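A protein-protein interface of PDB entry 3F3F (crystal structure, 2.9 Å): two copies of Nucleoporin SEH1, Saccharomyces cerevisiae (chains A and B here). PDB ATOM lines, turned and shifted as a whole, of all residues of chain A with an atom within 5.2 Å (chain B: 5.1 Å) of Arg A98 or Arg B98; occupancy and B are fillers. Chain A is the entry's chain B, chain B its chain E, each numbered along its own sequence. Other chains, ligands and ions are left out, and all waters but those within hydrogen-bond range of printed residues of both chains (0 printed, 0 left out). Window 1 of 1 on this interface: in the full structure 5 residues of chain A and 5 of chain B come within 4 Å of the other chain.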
ATOM      1  N   ASP A  51     -40.579 -33.382  19.364  1.00  0.00           N
ATOM      2  CA  ASP A  51     -39.131 -33.294  19.266  1.00  0.00           C
ATOM      3  C   ASP A  51     -38.494 -34.286  20.223  1.00  0.00           C
ATOM      4  O   ASP A  51     -39.027 -34.569  21.293  1.00  0.00           O
ATOM      5  CB  ASP A  51     -38.621 -31.873  19.593  1.00  0.00           C
ATOM      6  CG  ASP A  51     -37.194 -31.610  19.057  1.00  0.00           C
ATOM      7  OD1 ASP A  51     -36.450 -30.797  19.658  1.00  0.00           O
ATOM      8  OD2 ASP A  51     -36.823 -32.211  18.024  1.00  0.00           O
ATOM      9  N   TRP A  53     -34.387 -35.465  21.579  1.00  0.00           N
ATOM     10  CA  TRP A  53     -33.024 -34.975  21.583  1.00  0.00           C
ATOM     11  C   TRP A  53     -32.232 -35.600  22.725  1.00  0.00           C
ATOM     12  O   TRP A  53     -32.799 -36.005  23.740  1.00  0.00           O
ATOM     13  CB  TRP A  53     -33.020 -33.426  21.636  1.00  0.00           C
ATOM     14  CG  TRP A  53     -33.261 -32.783  22.977  1.00  0.00           C
ATOM     15  CD1 TRP A  53     -32.317 -32.483  23.927  1.00  0.00           C
ATOM     16  CD2 TRP A  53     -34.515 -32.356  23.515  1.00  0.00           C
ATOM     17  NE1 TRP A  53     -32.906 -31.895  25.023  1.00  0.00           N
ATOM     18  CE2 TRP A  53     -34.256 -31.806  24.801  1.00  0.00           C
ATOM     19  CE3 TRP A  53     -35.835 -32.388  23.048  1.00  0.00           C
ATOM     20  CZ2 TRP A  53     -35.273 -31.291  25.622  1.00  0.00           C
ATOM     21  CZ3 TRP A  53     -36.849 -31.877  23.868  1.00  0.00           C
ATOM     22  CH2 TRP A  53     -36.557 -31.337  25.139  1.00  0.00           C
ATOM     23  N   ASP A  89     -37.864 -23.308  21.422  1.00  0.00           N
ATOM     24  CA  ASP A  89     -37.681 -22.244  20.444  1.00  0.00           C
ATOM     25  C   ASP A  89     -38.657 -22.549  19.313  1.00  0.00           C
ATOM     26  O   ASP A  89     -38.365 -23.354  18.434  1.00  0.00           O
ATOM     27  CB  ASP A  89     -36.231 -22.228  19.923  1.00  0.00           C
ATOM     28  CG  ASP A  89     -36.029 -21.262  18.759  1.00  0.00           C
ATOM     29  OD1 ASP A  89     -36.574 -20.132  18.820  1.00  0.00           O
ATOM     30  OD2 ASP A  89     -35.319 -21.635  17.795  1.00  0.00           O
ATOM     31  N   GLN A  92     -38.153 -23.419  15.191  1.00  0.00           N
ATOM     32  CA  GLN A  92     -37.394 -24.581  14.745  1.00  0.00           C
ATOM     33  C   GLN A  92     -38.373 -25.668  14.332  1.00  0.00           C
ATOM     34  O   GLN A  92     -39.459 -25.785  14.902  1.00  0.00           O
ATOM     35  CB  GLN A  92     -36.499 -25.099  15.876  1.00  0.00           C
ATOM     36  CG  GLN A  92     -35.397 -24.145  16.272  1.00  0.00           C
ATOM     37  CD  GLN A  92     -34.370 -23.982  15.179  1.00  0.00           C
ATOM     38  OE1 GLN A  92     -33.691 -24.936  14.809  1.00  0.00           O
ATOM     39  NE2 GLN A  92     -34.253 -22.772  14.650  1.00  0.00           N
ATOM     40  N   SER A  96     -36.551 -31.839  14.728  1.00  0.00           N
ATOM     41  CA  SER A  96     -35.247 -31.377  14.276  1.00  0.00           C
ATOM     42  C   SER A  96     -34.150 -31.682  15.297  1.00  0.00           C
ATOM     43  O   SER A  96     -32.968 -31.634  14.965  1.00  0.00           O
ATOM     44  CB  SER A  96     -35.294 -29.872  13.989  1.00  0.00           C
ATOM     45  OG  SER A  96     -35.586 -29.126  15.154  1.00  0.00           O
ATOM     46  N   GLY A  97     -34.541 -32.015  16.527  1.00  0.00           N
ATOM     47  CA  GLY A  97     -33.568 -32.305  17.574  1.00  0.00           C
ATOM     48  C   GLY A  97     -32.976 -31.009  18.110  1.00  0.00           C
ATOM     49  O   GLY A  97     -32.181 -31.002  19.051  1.00  0.00           O
ATOM     50  N   ARG A  98     -33.401 -29.912  17.488  1.00  0.00           N
ATOM     51  CA  ARG A  98     -32.961 -28.553  17.795  1.00  0.00           C
ATOM     52  C   ARG A  98     -34.137 -27.705  18.228  1.00  0.00           C
ATOM     53  O   ARG A  98     -34.129 -26.496  17.992  1.00  0.00           O
ATOM     54  CB  ARG A  98     -32.412 -27.872  16.540  1.00  0.00           C
ATOM     55  CG  ARG A  98     -31.257 -28.542  15.850  1.00  0.00           C
ATOM     56  CD  ARG A  98     -31.090 -27.959  14.454  1.00  0.00           C
ATOM     57  NE  ARG A  98     -29.785 -28.267  13.878  1.00  0.00           N
ATOM     58  CZ  ARG A  98     -28.656 -27.655  14.221  1.00  0.00           C
ATOM     59  NH1 ARG A  98     -28.677 -26.694  15.140  1.00  0.00           N
ATOM     60  NH2 ARG A  98     -27.509 -28.005  13.650  1.00  0.00           N
ATOM     61  N   ARG A  99     -35.152 -28.296  18.844  1.00  0.00           N
ATOM     62  CA  ARG A  99     -36.305 -27.480  19.203  1.00  0.00           C
ATOM     63  C   ARG A  99     -36.261 -26.970  20.634  1.00  0.00           C
ATOM     64  O   ARG A  99     -36.966 -26.021  20.987  1.00  0.00           O
ATOM     65  CB  ARG A  99     -37.599 -28.254  18.930  1.00  0.00           C
ATOM     66  CG  ARG A  99     -38.836 -27.391  18.926  1.00  0.00           C
ATOM     67  CD  ARG A  99     -39.969 -28.069  18.187  1.00  0.00           C
ATOM     68  NE  ARG A  99     -41.243 -27.379  18.377  1.00  0.00           N
ATOM     69  CZ  ARG A  99     -41.478 -26.119  18.023  1.00  0.00           C
ATOM     70  NH1 ARG A  99     -40.522 -25.405  17.454  1.00  0.00           N
ATOM     71  NH2 ARG A  99     -42.666 -25.566  18.247  1.00  0.00           N
ATOM     72  N   TRP A 100     -35.412 -27.593  21.450  1.00  0.00           N
ATOM     73  CA  TRP A 100     -35.263 -27.193  22.847  1.00  0.00           C
ATOM     74  C   TRP A 100     -33.803 -26.844  23.191  1.00  0.00           C
ATOM     75  O   TRP A 100     -32.925 -27.717  23.163  1.00  0.00           O
ATOM     76  CB  TRP A 100     -35.778 -28.311  23.766  1.00  0.00           C
ATOM     77  CG  TRP A 100     -37.276 -28.498  23.700  1.00  0.00           C
ATOM     78  CD1 TRP A 100     -37.993 -29.088  22.696  1.00  0.00           C
ATOM     79  CD2 TRP A 100     -38.234 -28.063  24.668  1.00  0.00           C
ATOM     80  NE1 TRP A 100     -39.336 -29.043  22.977  1.00  0.00           N
ATOM     81  CE2 TRP A 100     -39.510 -28.418  24.183  1.00  0.00           C
ATOM     82  CE3 TRP A 100     -38.135 -27.403  25.899  1.00  0.00           C
ATOM     83  CZ2 TRP A 100     -40.680 -28.137  24.888  1.00  0.00           C
ATOM     84  CZ3 TRP A 100     -39.298 -27.125  26.602  1.00  0.00           C
ATOM     85  CH2 TRP A 100     -40.553 -27.491  26.093  1.00  0.00           C
ATOM     86  N   ASN A 101     -33.561 -25.568  23.515  1.00  0.00           N
ATOM     87  CA  ASN A 101     -32.225 -25.068  23.849  1.00  0.00           C
ATOM     88  C   ASN A 101     -31.898 -25.137  25.322  1.00  0.00           C
ATOM     89  O   ASN A 101     -32.660 -24.638  26.149  1.00  0.00           O
ATOM     90  CB  ASN A 101     -32.068 -23.604  23.444  1.00  0.00           C
ATOM     91  CG  ASN A 101     -32.456 -23.348  22.010  1.00  0.00           C
ATOM     92  OD1 ASN A 101     -33.634 -23.207  21.686  1.00  0.00           O
ATOM     93  ND2 ASN A 101     -31.464 -23.290  21.132  1.00  0.00           N
ATOM     94  N   LYS A 102     -30.754 -25.729  25.653  1.00  0.00           N
ATOM     95  CA  LYS A 102     -30.333 -25.797  27.050  1.00  0.00           C
ATOM     96  C   LYS A 102     -30.183 -24.355  27.559  1.00  0.00           C
ATOM     97  O   LYS A 102     -29.537 -23.519  26.925  1.00  0.00           O
ATOM     98  CB  LYS A 102     -28.986 -26.519  27.208  1.00  0.00           C
ATOM     99  CG  LYS A 102     -28.418 -26.377  28.626  1.00  0.00           C
ATOM    100  CD  LYS A 102     -26.915 -26.555  28.691  1.00  0.00           C
ATOM    101  CE  LYS A 102     -26.526 -28.002  28.900  1.00  0.00           C
ATOM    102  NZ  LYS A 102     -25.070 -28.142  29.204  1.00  0.00           N
ATOM    103  N   ASP B  51     -19.626 -34.041  12.165  1.00  0.00           N
ATOM    104  CA  ASP B  51     -21.047 -33.750  12.210  1.00  0.00           C
ATOM    105  C   ASP B  51     -21.560 -33.458  10.815  1.00  0.00           C
ATOM    106  O   ASP B  51     -20.853 -32.913   9.969  1.00  0.00           O
ATOM    107  CB  ASP B  51     -21.354 -32.551  13.108  1.00  0.00           C
ATOM    108  CG  ASP B  51     -22.821 -32.512  13.546  1.00  0.00           C
ATOM    109  OD1 ASP B  51     -23.371 -31.410  13.803  1.00  0.00           O
ATOM    110  OD2 ASP B  51     -23.422 -33.601  13.645  1.00  0.00           O
ATOM    111  N   TRP B  53     -25.393 -32.245   8.841  1.00  0.00           N
ATOM    112  CA  TRP B  53     -26.681 -31.667   9.159  1.00  0.00           C
ATOM    113  C   TRP B  53     -27.273 -30.988   7.941  1.00  0.00           C
ATOM    114  O   TRP B  53     -26.550 -30.573   7.040  1.00  0.00           O
ATOM    115  CB  TRP B  53     -26.554 -30.705  10.364  1.00  0.00           C
ATOM    116  CG  TRP B  53     -25.989 -29.320  10.091  1.00  0.00           C
ATOM    117  CD1 TRP B  53     -26.692 -28.206   9.731  1.00  0.00           C
ATOM    118  CD2 TRP B  53     -24.617 -28.911  10.170  1.00  0.00           C
ATOM    119  NE1 TRP B  53     -25.847 -27.130   9.582  1.00  0.00           N
ATOM    120  CE2 TRP B  53     -24.568 -27.537   9.841  1.00  0.00           C
ATOM    121  CE3 TRP B  53     -23.423 -29.571  10.478  1.00  0.00           C
ATOM    122  CZ2 TRP B  53     -23.373 -26.813   9.814  1.00  0.00           C
ATOM    123  CZ3 TRP B  53     -22.232 -28.845  10.448  1.00  0.00           C
ATOM    124  CH2 TRP B  53     -22.220 -27.484  10.117  1.00  0.00           C
ATOM    125  N   TRP B  86     -22.956 -20.447  11.148  1.00  0.00           N
ATOM    126  CA  TRP B  86     -23.086 -21.432  12.208  1.00  0.00           C
ATOM    127  C   TRP B  86     -21.911 -21.399  13.153  1.00  0.00           C
ATOM    128  O   TRP B  86     -20.810 -21.058  12.760  1.00  0.00           O
ATOM    129  CB  TRP B  86     -23.190 -22.826  11.600  1.00  0.00           C
ATOM    130  CG  TRP B  86     -23.957 -22.852  10.321  1.00  0.00           C
ATOM    131  CD1 TRP B  86     -23.543 -22.386   9.109  1.00  0.00           C
ATOM    132  CD2 TRP B  86     -25.290 -23.338  10.130  1.00  0.00           C
ATOM    133  NE1 TRP B  86     -24.533 -22.548   8.172  1.00  0.00           N
ATOM    134  CE2 TRP B  86     -25.619 -23.128   8.771  1.00  0.00           C
ATOM    135  CE3 TRP B  86     -26.246 -23.924  10.975  1.00  0.00           C
ATOM    136  CZ2 TRP B  86     -26.858 -23.486   8.238  1.00  0.00           C
ATOM    137  CZ3 TRP B  86     -27.471 -24.276  10.447  1.00  0.00           C
ATOM    138  CH2 TRP B  86     -27.769 -24.055   9.091  1.00  0.00           C
ATOM    139  N   GLN B  92     -21.962 -30.860  22.508  1.00  0.00           N
ATOM    140  CA  GLN B  92     -22.894 -31.726  21.803  1.00  0.00           C
ATOM    141  C   GLN B  92     -22.121 -32.890  21.234  1.00  0.00           C
ATOM    142  O   GLN B  92     -20.964 -32.746  20.865  1.00  0.00           O
ATOM    143  CB  GLN B  92     -23.578 -30.968  20.659  1.00  0.00           C
ATOM    144  CG  GLN B  92     -24.511 -29.858  21.107  1.00  0.00           C
ATOM    145  CD  GLN B  92     -25.736 -30.382  21.832  1.00  0.00           C
ATOM    146  OE1 GLN B  92     -26.573 -31.075  21.247  1.00  0.00           O
ATOM    147  NE2 GLN B  92     -25.846 -30.057  23.115  1.00  0.00           N
ATOM    148  N   SER B  96     -24.345 -35.866  15.945  1.00  0.00           N
ATOM    149  CA  SER B  96     -25.669 -35.672  16.504  1.00  0.00           C
ATOM    150  C   SER B  96     -26.567 -34.834  15.584  1.00  0.00           C
ATOM    151  O   SER B  96     -27.782 -34.795  15.765  1.00  0.00           O
ATOM    152  CB  SER B  96     -25.564 -35.016  17.884  1.00  0.00           C
ATOM    153  OG  SER B  96     -24.995 -33.724  17.801  1.00  0.00           O
ATOM    154  N   GLY B  97     -25.982 -34.180  14.586  1.00  0.00           N
ATOM    155  CA  GLY B  97     -26.781 -33.364  13.687  1.00  0.00           C
ATOM    156  C   GLY B  97     -27.108 -32.036  14.337  1.00  0.00           C
ATOM    157  O   GLY B  97     -27.684 -31.133  13.729  1.00  0.00           O
ATOM    158  N   ARG B  98     -26.757 -31.924  15.604  1.00  0.00           N
ATOM    159  CA  ARG B  98     -26.982 -30.687  16.296  1.00  0.00           C
ATOM    160  C   ARG B  98     -25.710 -30.284  17.016  1.00  0.00           C
ATOM    161  O   ARG B  98     -25.698 -30.154  18.239  1.00  0.00           O
ATOM    162  CB  ARG B  98     -28.124 -30.800  17.297  1.00  0.00           C
ATOM    163  CG  ARG B  98     -28.438 -29.455  17.889  1.00  0.00           C
ATOM    164  CD  ARG B  98     -29.330 -29.528  19.075  1.00  0.00           C
ATOM    165  NE  ARG B  98     -29.311 -28.234  19.737  1.00  0.00           N
ATOM    166  CZ  ARG B  98     -30.123 -27.878  20.726  1.00  0.00           C
ATOM    167  NH1 ARG B  98     -31.041 -28.732  21.183  1.00  0.00           N
ATOM    168  NH2 ARG B  98     -30.011 -26.661  21.258  1.00  0.00           N
ATOM    169  N   ARG B  99     -24.626 -30.130  16.258  1.00  0.00           N
ATOM    170  CA  ARG B  99     -23.362 -29.689  16.841  1.00  0.00           C
ATOM    171  C   ARG B  99     -23.070 -28.262  16.385  1.00  0.00           C
ATOM    172  O   ARG B  99     -22.245 -27.569  16.979  1.00  0.00           O
ATOM    173  CB  ARG B  99     -22.213 -30.624  16.447  1.00  0.00           C
ATOM    174  CG  ARG B  99     -20.915 -30.362  17.210  1.00  0.00           C
ATOM    175  CD  ARG B  99     -19.996 -31.578  17.179  1.00  0.00           C
ATOM    176  NE  ARG B  99     -18.666 -31.286  17.712  1.00  0.00           N
ATOM    177  CZ  ARG B  99     -18.420 -30.850  18.944  1.00  0.00           C
ATOM    178  NH1 ARG B  99     -19.414 -30.650  19.794  1.00  0.00           N
ATOM    179  NH2 ARG B  99     -17.177 -30.602  19.328  1.00  0.00           N
ATOM    180  N   TRP B 100     -23.771 -27.825  15.344  1.00  0.00           N
ATOM    181  CA  TRP B 100     -23.595 -26.480  14.821  1.00  0.00           C
ATOM    182  C   TRP B 100     -24.909 -25.694  14.802  1.00  0.00           C
ATOM    183  O   TRP B 100     -25.834 -26.051  14.070  1.00  0.00           O
ATOM    184  CB  TRP B 100     -22.990 -26.547  13.412  1.00  0.00           C
ATOM    185  CG  TRP B 100     -21.549 -27.025  13.389  1.00  0.00           C
ATOM    186  CD1 TRP B 100     -21.103 -28.307  13.548  1.00  0.00           C
ATOM    187  CD2 TRP B 100     -20.379 -26.216  13.214  1.00  0.00           C
ATOM    188  NE1 TRP B 100     -19.734 -28.345  13.480  1.00  0.00           N
ATOM    189  CE2 TRP B 100     -19.264 -27.075  13.277  1.00  0.00           C
ATOM    190  CE3 TRP B 100     -20.168 -24.845  13.012  1.00  0.00           C
ATOM    191  CZ2 TRP B 100     -17.957 -26.610  13.143  1.00  0.00           C
ATOM    192  CZ3 TRP B 100     -18.871 -24.386  12.879  1.00  0.00           C
ATOM    193  CH2 TRP B 100     -17.781 -25.265  12.946  1.00  0.00           C
ATOM    194  N   ASN B 101     -24.978 -24.625  15.600  1.00  0.00           N
ATOM    195  CA  ASN B 101     -26.179 -23.787  15.706  1.00  0.00           C
ATOM    196  C   ASN B 101     -26.196 -22.631  14.732  1.00  0.00           C
ATOM    197  O   ASN B 101     -25.227 -21.888  14.644  1.00  0.00           O
ATOM    198  CB  ASN B 101     -26.312 -23.183  17.104  1.00  0.00           C
ATOM    199  CG  ASN B 101     -26.187 -24.202  18.194  1.00  0.00           C
ATOM    200  OD1 ASN B 101     -25.082 -24.580  18.573  1.00  0.00           O
ATOM    201  ND2 ASN B 101     -27.321 -24.668  18.703  1.00  0.00           N
ATOM    202  N   LYS B 102     -27.304 -22.458  14.018  1.00  0.00           N
ATOM    203  CA  LYS B 102     -27.419 -21.344  13.090  1.00  0.00           C
ATOM    204  C   LYS B 102     -27.347 -20.064  13.924  1.00  0.00           C
ATOM    205  O   LYS B 102     -28.039 -19.934  14.933  1.00  0.00           O
ATOM    206  CB  LYS B 102     -28.750 -21.383  12.336  1.00  0.00           C
ATOM    207  CG  LYS B 102     -29.005 -20.104  11.560  1.00  0.00           C
ATOM    208  CD  LYS B 102     -30.480 -19.842  11.299  1.00  0.00           C
ATOM    209  CE  LYS B 102     -30.932 -20.447   9.984  1.00  0.00           C
ATOM    210  NZ  LYS B 102     -32.295 -19.971   9.595  1.00  0.00           N
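CG of Arg B98 touches CG of Arg A98 (3.6 Å). Arg A98 touches Asn B101 (NH1 to CA, 3.9 Å). Arg B98 touches Asn A101 (NH2 to ND2, 3.7 Å).
Gly A97 touches Arg B98, and with the chains exchanged Arg A98 touches Gly B97. Arg A98 touches its own counterpart, Arg B98. Arg A98 touches Trp B100, and with the chains exchanged Trp A100 touches Arg B98. Arg A98 touches Asn B101, and with the chains exchanged Asn A101 touches Arg B98. 10 positions are printed for both chains. Of the 7 pairs that touch across the chains among the printed residues, 7 have their exchanged pair printed and touching as well.
The backbone carbonyl oxygen (O) of Gly B97 is in hydrogen-bond range of the guanidinium group (NH2) of Arg A98 (3.1 Å). The backbone carbonyl oxygen of Trp A100 sits at hydrogen-bond distance from the guanidinium group of Arg B98, at 2.9 Å. The guanidinium group of Arg B98 sits close to the backbone carbonyl oxygen of Gly A97 (3.3 Å). The backbone carbonyl oxygen of Trp B100 sits at hydrogen-bond distance from the guanidinium group of Arg A98, 2.6 Å away.
Among the printed residues, 7 pairs touch across the chains.
The backbone NH of Arg A98 lies close to the side-chain hydroxyl of Ser A96 (3.3 Å). The backbone carbonyl oxygen (O) of Arg B98 sits close to the side-chain amide oxygen (OE1) of Gln B92 (3.3 Å). OD2 of Asp B51 sits at hydrogen-bond distance from N of Gly B97 (2.8 Å). The backbone NH (N) of Arg B98 sits close to the side-chain hydroxyl (OG) of Ser B96. OD2 of Asp A51 lies within hydrogen-bond range of N of Gly A97, 2.7 Å away.
Of the printed residues of chain B, Arg A98 touches Gly B97 (3.1 Å), Arg B98 (3.6 Å), Trp B100 (2.6 Å) and Asn B101 (3.9 Å). Of chain A, only Gly A97 (3.2 Å), Arg A98 (3.6 Å), Trp A100 (2.9 Å) and Asn A101 (3.7 Å) come within 4 Å of Arg B98. Of the printed residues of chain B, Gly A97 touches Arg B98. Printed residues of chain A within 4 Å of Trp B100: Arg A98. Printed residues of chain B within 4 Å of Trp A100: Arg B98 (2.9 Å). Gln B92 touches none of the printed residues of chain A. The nearest printed residue of chain B that does not touch Arg A98 is Trp B53 (4.01 Å). The nearest residue of chain A that does not touch Arg B98 is Lys A102 (4.6 Å).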
